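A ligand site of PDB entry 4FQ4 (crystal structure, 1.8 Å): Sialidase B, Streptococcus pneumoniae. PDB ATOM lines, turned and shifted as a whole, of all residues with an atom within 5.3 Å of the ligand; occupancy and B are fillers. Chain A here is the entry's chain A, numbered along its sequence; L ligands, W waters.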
ATOM      1  N   ARG A 245      11.950  -7.050  -8.990  1.00  0.00           N
ATOM      2  CA  ARG A 245      11.041  -6.186  -8.226  1.00  0.00           C
ATOM      3  C   ARG A 245       9.614  -6.404  -8.690  1.00  0.00           C
ATOM      4  O   ARG A 245       9.376  -6.972  -9.758  1.00  0.00           O
ATOM      5  CB  ARG A 245      11.417  -4.695  -8.383  1.00  0.00           C
ATOM      6  CG  ARG A 245      12.547  -4.207  -7.441  1.00  0.00           C
ATOM      7  CD  ARG A 245      12.375  -2.714  -7.071  1.00  0.00           C
ATOM      8  NE  ARG A 245      11.087  -2.483  -6.406  1.00  0.00           N
ATOM      9  CZ  ARG A 245      10.584  -1.273  -6.171  1.00  0.00           C
ATOM     10  NH1 ARG A 245      11.271  -0.189  -6.524  1.00  0.00           N
ATOM     11  NH2 ARG A 245       9.396  -1.162  -5.574  1.00  0.00           N
ATOM     12  N   ILE A 246       8.660  -5.921  -7.903  1.00  0.00           N
ATOM     13  CA  ILE A 246       7.248  -5.900  -8.290  1.00  0.00           C
ATOM     14  C   ILE A 246       6.650  -7.314  -8.487  1.00  0.00           C
ATOM     15  O   ILE A 246       6.243  -7.670  -9.592  1.00  0.00           O
ATOM     16  CB  ILE A 246       7.000  -5.020  -9.566  1.00  0.00           C
ATOM     17  CG1 ILE A 246       7.955  -3.817  -9.633  1.00  0.00           C
ATOM     18  CG2 ILE A 246       5.572  -4.510  -9.594  1.00  0.00           C
ATOM     19  CD1 ILE A 246       7.810  -2.767  -8.486  1.00  0.00           C
ATOM     20  N   ASP A 270      13.846   1.643 -11.504  1.00  0.00           N
ATOM     21  CA  ASP A 270      12.657   1.661 -12.371  1.00  0.00           C
ATOM     22  C   ASP A 270      13.136   2.092 -13.752  1.00  0.00           C
ATOM     23  O   ASP A 270      14.180   2.739 -13.869  1.00  0.00           O
ATOM     24  CB  ASP A 270      11.638   2.729 -11.933  1.00  0.00           C
ATOM     25  CG  ASP A 270      10.927   2.422 -10.619  1.00  0.00           C
ATOM     26  OD1 ASP A 270      10.165   3.308 -10.177  1.00  0.00           O
ATOM     27  OD2 ASP A 270      11.114   1.315 -10.054  1.00  0.00           O
ATOM     28  N   SER A 271      12.387   1.774 -14.809  1.00  0.00           N
ATOM     29  CA  SER A 271      12.660   2.385 -16.126  1.00  0.00           C
ATOM     30  C   SER A 271      12.974   3.907 -16.035  1.00  0.00           C
ATOM     31  O   SER A 271      12.368   4.594 -15.221  1.00  0.00           O
ATOM     32  CB  SER A 271      11.476   2.167 -17.062  1.00  0.00           C
ATOM     33  OG  SER A 271      11.178   0.791 -17.194  1.00  0.00           O
ATOM     34  N   LYS A 272      13.900   4.442 -16.844  1.00  0.00           N
ATOM     35  CA  LYS A 272      14.634   3.731 -17.895  1.00  0.00           C
ATOM     36  C   LYS A 272      15.668   2.703 -17.408  1.00  0.00           C
ATOM     37  O   LYS A 272      16.460   2.953 -16.503  1.00  0.00           O
ATOM     38  CB  LYS A 272      15.316   4.745 -18.827  1.00  0.00           C
ATOM     39  CG  LYS A 272      16.385   5.604 -18.163  1.00  0.00           C
ATOM     40  CD  LYS A 272      16.854   6.735 -19.072  1.00  0.00           C
ATOM     41  CE  LYS A 272      18.040   7.498 -18.459  1.00  0.00           C
ATOM     42  NZ  LYS A 272      18.510   8.646 -19.302  1.00  0.00           N
ATOM     43  N   ILE A 326       7.460  -2.655 -17.277  1.00  0.00           N
ATOM     44  CA  ILE A 326       7.506  -2.420 -15.834  1.00  0.00           C
ATOM     45  C   ILE A 326       6.108  -2.530 -15.265  1.00  0.00           C
ATOM     46  O   ILE A 326       5.163  -2.097 -15.913  1.00  0.00           O
ATOM     47  CB  ILE A 326       8.172  -1.045 -15.484  1.00  0.00           C
ATOM     48  CG1 ILE A 326       8.153  -0.791 -13.975  1.00  0.00           C
ATOM     49  CG2 ILE A 326       7.510   0.117 -16.241  1.00  0.00           C
ATOM     50  CD1 ILE A 326       9.055   0.393 -13.555  1.00  0.00           C
ATOM     51  N   ASP A 327       5.994  -3.137 -14.078  1.00  0.00           N
ATOM     52  CA  ASP A 327       4.713  -3.241 -13.346  1.00  0.00           C
ATOM     53  C   ASP A 327       3.681  -4.138 -14.045  1.00  0.00           C
ATOM     54  O   ASP A 327       2.856  -3.654 -14.818  1.00  0.00           O
ATOM     55  CB  ASP A 327       4.070  -1.867 -13.124  1.00  0.00           C
ATOM     56  CG  ASP A 327       4.813  -1.014 -12.109  1.00  0.00           C
ATOM     57  OD1 ASP A 327       5.714  -1.528 -11.421  1.00  0.00           O
ATOM     58  OD2 ASP A 327       4.471   0.202 -12.014  1.00  0.00           O
ATOM     59  N   ASP A 344       3.144  -2.117 -18.018  1.00  0.00           N
ATOM     60  CA  ASP A 344       3.484  -0.869 -18.710  1.00  0.00           C
ATOM     61  C   ASP A 344       4.583  -1.177 -19.727  1.00  0.00           C
ATOM     62  O   ASP A 344       5.391  -2.091 -19.517  1.00  0.00           O
ATOM     63  CB  ASP A 344       4.014   0.207 -17.754  1.00  0.00           C
ATOM     64  CG  ASP A 344       3.033   0.582 -16.651  1.00  0.00           C
ATOM     65  OD1 ASP A 344       1.799   0.489 -16.830  1.00  0.00           O
ATOM     66  OD2 ASP A 344       3.526   1.013 -15.584  1.00  0.00           O
ATOM     67  N   MET A 346       7.706   0.809 -22.078  1.00  0.00           N
ATOM     68  CA  MET A 346       8.476   2.039 -22.293  1.00  0.00           C
ATOM     69  C   MET A 346       9.386   1.855 -23.500  1.00  0.00           C
ATOM     70  O   MET A 346      10.138   0.885 -23.566  1.00  0.00           O
ATOM     71  CB  MET A 346       9.386   2.273 -21.090  1.00  0.00           C
ATOM     72  CG  MET A 346       8.693   2.228 -19.761  1.00  0.00           C
ATOM     73  SD  MET A 346       7.806   3.758 -19.499  1.00  0.00           S
ATOM     74  CE  MET A 346       6.368   3.072 -18.686  1.00  0.00           C
ATOM     75  N   GLY A 351      11.216   6.367 -19.128  1.00  0.00           N
ATOM     76  CA  GLY A 351      10.592   5.996 -17.869  1.00  0.00           C
ATOM     77  C   GLY A 351       9.579   7.059 -17.461  1.00  0.00           C
ATOM     78  O   GLY A 351       9.189   7.906 -18.278  1.00  0.00           O
ATOM     79  N   ASN A 352       9.144   7.000 -16.201  1.00  0.00           N
ATOM     80  CA  ASN A 352       8.209   7.959 -15.614  1.00  0.00           C
ATOM     81  C   ASN A 352       8.746   9.382 -15.730  1.00  0.00           C
ATOM     82  O   ASN A 352       8.027  10.308 -16.133  1.00  0.00           O
ATOM     83  CB  ASN A 352       7.972   7.604 -14.139  1.00  0.00           C
ATOM     84  CG  ASN A 352       6.953   8.512 -13.436  1.00  0.00           C
ATOM     85  OD1 ASN A 352       7.009   9.736 -13.534  1.00  0.00           O
ATOM     86  ND2 ASN A 352       6.037   7.888 -12.687  1.00  0.00           N
ATOM     87  N   ASN A 353      10.016   9.547 -15.352  1.00  0.00           N
ATOM     88  CA  ASN A 353      10.680  10.848 -15.338  1.00  0.00           C
ATOM     89  C   ASN A 353      10.566  11.624 -16.659  1.00  0.00           C
ATOM     90  O   ASN A 353      10.254  12.822 -16.672  1.00  0.00           O
ATOM     91  CB  ASN A 353      12.155  10.678 -14.970  1.00  0.00           C
ATOM     92  CG  ASN A 353      12.955  11.967 -15.116  1.00  0.00           C
ATOM     93  OD1 ASN A 353      12.498  13.052 -14.746  1.00  0.00           O
ATOM     94  ND2 ASN A 353      14.156  11.861 -15.667  1.00  0.00           N
ATOM     95  N   TYR A 489      -1.058   4.469 -15.601  1.00  0.00           N
ATOM     96  CA  TYR A 489      -0.069   3.522 -15.108  1.00  0.00           C
ATOM     97  C   TYR A 489      -0.732   2.312 -14.489  1.00  0.00           C
ATOM     98  O   TYR A 489      -1.611   2.436 -13.638  1.00  0.00           O
ATOM     99  CB  TYR A 489       0.831   4.204 -14.076  1.00  0.00           C
ATOM    100  CG  TYR A 489       1.723   5.235 -14.709  1.00  0.00           C
ATOM    101  CD1 TYR A 489       2.895   4.862 -15.332  1.00  0.00           C
ATOM    102  CD2 TYR A 489       1.368   6.576 -14.708  1.00  0.00           C
ATOM    103  CE1 TYR A 489       3.720   5.788 -15.925  1.00  0.00           C
ATOM    104  CE2 TYR A 489       2.183   7.527 -15.301  1.00  0.00           C
ATOM    105  CZ  TYR A 489       3.348   7.121 -15.910  1.00  0.00           C
ATOM    106  OH  TYR A 489       4.191   8.032 -16.510  1.00  0.00           O
ATOM    107  N   TYR A 509      -3.686   3.979 -12.591  1.00  0.00           N
ATOM    108  CA  TYR A 509      -3.782   5.299 -11.976  1.00  0.00           C
ATOM    109  C   TYR A 509      -3.190   6.391 -12.863  1.00  0.00           C
ATOM    110  O   TYR A 509      -2.327   6.152 -13.712  1.00  0.00           O
ATOM    111  CB  TYR A 509      -3.116   5.330 -10.590  1.00  0.00           C
ATOM    112  CG  TYR A 509      -1.620   5.057 -10.607  1.00  0.00           C
ATOM    113  CD1 TYR A 509      -0.705   6.096 -10.705  1.00  0.00           C
ATOM    114  CD2 TYR A 509      -1.136   3.766 -10.509  1.00  0.00           C
ATOM    115  CE1 TYR A 509       0.662   5.837 -10.718  1.00  0.00           C
ATOM    116  CE2 TYR A 509       0.218   3.501 -10.527  1.00  0.00           C
ATOM    117  CZ  TYR A 509       1.116   4.548 -10.630  1.00  0.00           C
ATOM    118  OH  TYR A 509       2.477   4.278 -10.635  1.00  0.00           O
ATOM    119  N   THR A 539       1.312   8.197  -6.811  1.00  0.00           N
ATOM    120  CA  THR A 539       1.504   6.828  -7.276  1.00  0.00           C
ATOM    121  C   THR A 539       0.418   6.006  -6.582  1.00  0.00           C
ATOM    122  O   THR A 539       0.665   5.353  -5.575  1.00  0.00           O
ATOM    123  CB  THR A 539       2.902   6.324  -6.899  1.00  0.00           C
ATOM    124  OG1 THR A 539       3.882   7.232  -7.425  1.00  0.00           O
ATOM    125  CG2 THR A 539       3.167   4.924  -7.440  1.00  0.00           C
ATOM    126  N   GLU A 541      -1.180   3.220  -6.472  1.00  0.00           N
ATOM    127  CA  GLU A 541      -1.255   1.799  -6.762  1.00  0.00           C
ATOM    128  C   GLU A 541      -2.407   1.196  -5.967  1.00  0.00           C
ATOM    129  O   GLU A 541      -2.474   1.335  -4.728  1.00  0.00           O
ATOM    130  CB  GLU A 541       0.079   1.129  -6.414  1.00  0.00           C
ATOM    131  CG  GLU A 541       1.222   1.533  -7.373  1.00  0.00           C
ATOM    132  CD  GLU A 541       2.584   1.448  -6.724  1.00  0.00           C
ATOM    133  OE1 GLU A 541       3.608   1.372  -7.451  1.00  0.00           O
ATOM    134  OE2 GLU A 541       2.643   1.463  -5.482  1.00  0.00           O
ATOM    135  N   ARG A 557      -2.536   3.072  -2.357  1.00  0.00           N
ATOM    136  CA  ARG A 557      -1.441   3.879  -1.840  1.00  0.00           C
ATOM    137  C   ARG A 557      -1.715   5.368  -2.038  1.00  0.00           C
ATOM    138  O   ARG A 557      -2.242   5.770  -3.067  1.00  0.00           O
ATOM    139  CB  ARG A 557      -0.155   3.462  -2.591  1.00  0.00           C
ATOM    140  CG  ARG A 557       1.086   4.306  -2.319  1.00  0.00           C
ATOM    141  CD  ARG A 557       2.208   3.824  -3.234  1.00  0.00           C
ATOM    142  NE  ARG A 557       3.390   4.687  -3.231  1.00  0.00           N
ATOM    143  CZ  ARG A 557       4.529   4.377  -3.835  1.00  0.00           C
ATOM    144  NH1 ARG A 557       4.635   3.230  -4.510  1.00  0.00           N
ATOM    145  NH2 ARG A 557       5.554   5.211  -3.789  1.00  0.00           N
ATOM    146  N   GLY A 590       4.499   6.357   0.481  1.00  0.00           N
ATOM    147  CA  GLY A 590       3.597   5.213   0.350  1.00  0.00           C
ATOM    148  C   GLY A 590       4.251   3.972  -0.221  1.00  0.00           C
ATOM    149  O   GLY A 590       5.376   4.012  -0.714  1.00  0.00           O
ATOM    150  N   ARG A 619      10.231   1.449   4.432  1.00  0.00           N
ATOM    151  CA  ARG A 619       9.539   0.239   3.979  1.00  0.00           C
ATOM    152  C   ARG A 619      10.041  -0.945   4.800  1.00  0.00           C
ATOM    153  O   ARG A 619      10.989  -1.619   4.419  1.00  0.00           O
ATOM    154  CB  ARG A 619       9.704   0.040   2.468  1.00  0.00           C
ATOM    155  CG  ARG A 619       9.039   1.155   1.641  1.00  0.00           C
ATOM    156  CD  ARG A 619       9.150   0.932   0.132  1.00  0.00           C
ATOM    157  NE  ARG A 619       8.215   1.777  -0.610  1.00  0.00           N
ATOM    158  CZ  ARG A 619       8.316   2.053  -1.904  1.00  0.00           C
ATOM    159  NH1 ARG A 619       9.329   1.565  -2.621  1.00  0.00           N
ATOM    160  NH2 ARG A 619       7.413   2.829  -2.497  1.00  0.00           N
ATOM    161  N   TYR A 653       7.110  -3.889  -1.698  1.00  0.00           N
ATOM    162  CA  TYR A 653       5.993  -4.332  -2.526  1.00  0.00           C
ATOM    163  C   TYR A 653       5.714  -5.795  -2.220  1.00  0.00           C
ATOM    164  O   TYR A 653       6.630  -6.529  -1.828  1.00  0.00           O
ATOM    165  CB  TYR A 653       6.277  -4.156  -4.007  1.00  0.00           C
ATOM    166  CG  TYR A 653       6.089  -2.741  -4.536  1.00  0.00           C
ATOM    167  CD1 TYR A 653       6.555  -1.641  -3.817  1.00  0.00           C
ATOM    168  CD2 TYR A 653       5.502  -2.522  -5.763  1.00  0.00           C
ATOM    169  CE1 TYR A 653       6.408  -0.347  -4.316  1.00  0.00           C
ATOM    170  CE2 TYR A 653       5.348  -1.246  -6.266  1.00  0.00           C
ATOM    171  CZ  TYR A 653       5.811  -0.155  -5.550  1.00  0.00           C
ATOM    172  OH  TYR A 653       5.648   1.117  -6.067  1.00  0.00           O
ATOM    173  N   SER A 673      12.808  -0.952  -0.639  1.00  0.00           N
ATOM    174  CA  SER A 673      12.996  -0.647  -2.050  1.00  0.00           C
ATOM    175  C   SER A 673      12.889   0.850  -2.364  1.00  0.00           C
ATOM    176  O   SER A 673      12.921   1.244  -3.539  1.00  0.00           O
ATOM    177  CB  SER A 673      12.039  -1.476  -2.928  1.00  0.00           C
ATOM    178  OG  SER A 673      10.678  -1.165  -2.676  1.00  0.00           O
ATOM    179  N   TRP A 674      12.774   1.674  -1.321  1.00  0.00           N
ATOM    180  CA  TRP A 674      12.826   3.142  -1.474  1.00  0.00           C
ATOM    181  C   TRP A 674      14.228   3.648  -1.131  1.00  0.00           C
ATOM    182  O   TRP A 674      14.792   4.483  -1.857  1.00  0.00           O
ATOM    183  CB  TRP A 674      11.790   3.822  -0.562  1.00  0.00           C
ATOM    184  CG  TRP A 674      11.654   5.324  -0.800  1.00  0.00           C
ATOM    185  CD1 TRP A 674      12.288   6.327  -0.116  1.00  0.00           C
ATOM    186  CD2 TRP A 674      10.840   5.964  -1.793  1.00  0.00           C
ATOM    187  NE1 TRP A 674      11.913   7.553  -0.619  1.00  0.00           N
ATOM    188  CE2 TRP A 674      11.030   7.355  -1.651  1.00  0.00           C
ATOM    189  CE3 TRP A 674       9.967   5.501  -2.780  1.00  0.00           C
ATOM    190  CZ2 TRP A 674      10.362   8.291  -2.458  1.00  0.00           C
ATOM    191  CZ3 TRP A 674       9.317   6.422  -3.595  1.00  0.00           C
ATOM    192  CH2 TRP A 674       9.518   7.803  -3.429  1.00  0.00           C
HETATM  193  O1  LIG L   1       7.606   3.499  -5.199  1.00  0.00           O
HETATM  194  S1  LIG L   1       8.760   3.024  -6.009  1.00  0.00           S
HETATM  195  O2  LIG L   1       9.553   2.018  -5.288  1.00  0.00           O
HETATM  196  O3  LIG L   1       9.596   4.119  -6.315  1.00  0.00           O
HETATM  197  C1  LIG L   1       8.170   2.370  -7.511  1.00  0.00           C
HETATM  198  C2  LIG L   1       7.322   3.344  -8.380  1.00  0.00           C
HETATM  199  N1  LIG L   1       7.151   2.947  -9.775  1.00  0.00           N
HETATM  200  C3  LIG L   1       6.357   3.892 -10.514  1.00  0.00           C
HETATM  201  C4  LIG L   1       6.566   3.774 -11.970  1.00  0.00           C
HETATM  202  C5  LIG L   1       7.827   4.164 -12.495  1.00  0.00           C
HETATM  203  C6  LIG L   1       8.054   4.039 -13.904  1.00  0.00           C
HETATM  204  C7  LIG L   1       9.356   4.439 -14.489  1.00  0.00           C
HETATM  205  C8  LIG L   1       7.070   3.538 -14.740  1.00  0.00           C
HETATM  206  F1  LIG L   1       7.313   3.453 -15.971  1.00  0.00           F
HETATM  207  C9  LIG L   1       5.812   3.126 -14.217  1.00  0.00           C
HETATM  208  C10 LIG L   1       5.569   3.244 -12.803  1.00  0.00           C
HETATM  209  O   HOH W   1       6.165   0.450  -9.348  1.00  0.00           O
HETATM  210  O   HOH W   2      11.674   3.250  -7.732  1.00  0.00           O
HETATM  211  O   HOH W   3       4.340   6.749 -10.607  1.00  0.00           O
HETATM  212  O   HOH W   4       9.189   6.714  -7.210  1.00  0.00           O
HETATM  213  O   HOH W   5      12.473   3.597  -5.202  1.00  0.00           O
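O2 of the ligand lies within salt-bridge range of NH1 of Arg 619 (2.7 Å).
The guanidinium group (NH2) of Arg 557 lies within salt-bridge range of an oxygen (O1) of the ligand (3.0 Å).
The guanidinium group of Arg 245 is in salt-bridge range of an oxygen (O2) of the ligand, at 3.1 Å.
A nitrogen (N1) of the ligand lies within salt-bridge range of the side-chain carboxylate (OD1) of Asp 270, 3.1 Å away.
The side-chain hydroxyl (OH) of Tyr 653 lies close to an oxygen (O1) of the ligand.
NH1 of Arg 619 lies within hydrogen-bond range of OG of Ser 673.
The backbone carbonyl oxygen (O) of Gly 590 is in hydrogen-bond range of the guanidinium group (NH2) of Arg 619, 3.0 Å away.
The guanidinium group of Arg 557 lies within hydrogen-bond range of the side-chain hydroxyl of Tyr 653, at 2.8 Å.
O of Gly 590 sits close to NE of Arg 557.
NH1 of Arg 245 is in salt-bridge range of OD2 of Asp 270.
OH of Tyr 653 lies within hydrogen-bond range of OE1 of Glu 541 (2.5 Å).
The backbone NH of Asp 344 is in hydrogen-bond range of the backbone carbonyl oxygen of Ile 326 (2.9 Å).
O of Tyr 489 sits at hydrogen-bond distance from N of Tyr 509.
The side-chain sulfur (SD) of Met 346 lies close to a fluorine (F1) of the ligand (3.6 Å).
O of Ser 271 touches C7 of the ligand, at 3.1 Å.
CG2 of Ile 326 touches F1 of the ligand, 3.4 Å away.
OD2 of Asp 327 touches C10 of the ligand, at 3.3 Å.
Asp 344 touches the ligand.
Gly 351 touches the ligand (CA to C7, 3.9 Å).
Asn 352 touches the ligand.
Tyr 489 touches the ligand.
Tyr 509 touches the ligand.
Ser 673 touches the ligand.
Trp 674 touches the ligand.
Water W2 bridges an oxygen (O3) of the ligand and the side-chain carboxylate (OD1) of Asp 270.
Water W1 lies within hydrogen-bond range of a nitrogen (N1) of the ligand (2.7 Å), the side-chain carboxylate (OD1) of Asp 327 (2.9 Å), the side-chain carboxylate (OE1) of Glu 541 (3.3 Å) and the side-chain hydroxyl (OH) of Tyr 653 (3.4 Å).
Water W5 bridges the backbone carbonyl oxygen of Ser 673 and an oxygen (O3) of the ligand.
Water W3 lies within hydrogen-bond range of ND2 of Asn 352 (2.9 Å), OH of Tyr 509 (3.1 Å) and OG1 of Thr 539 (3.3 Å).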
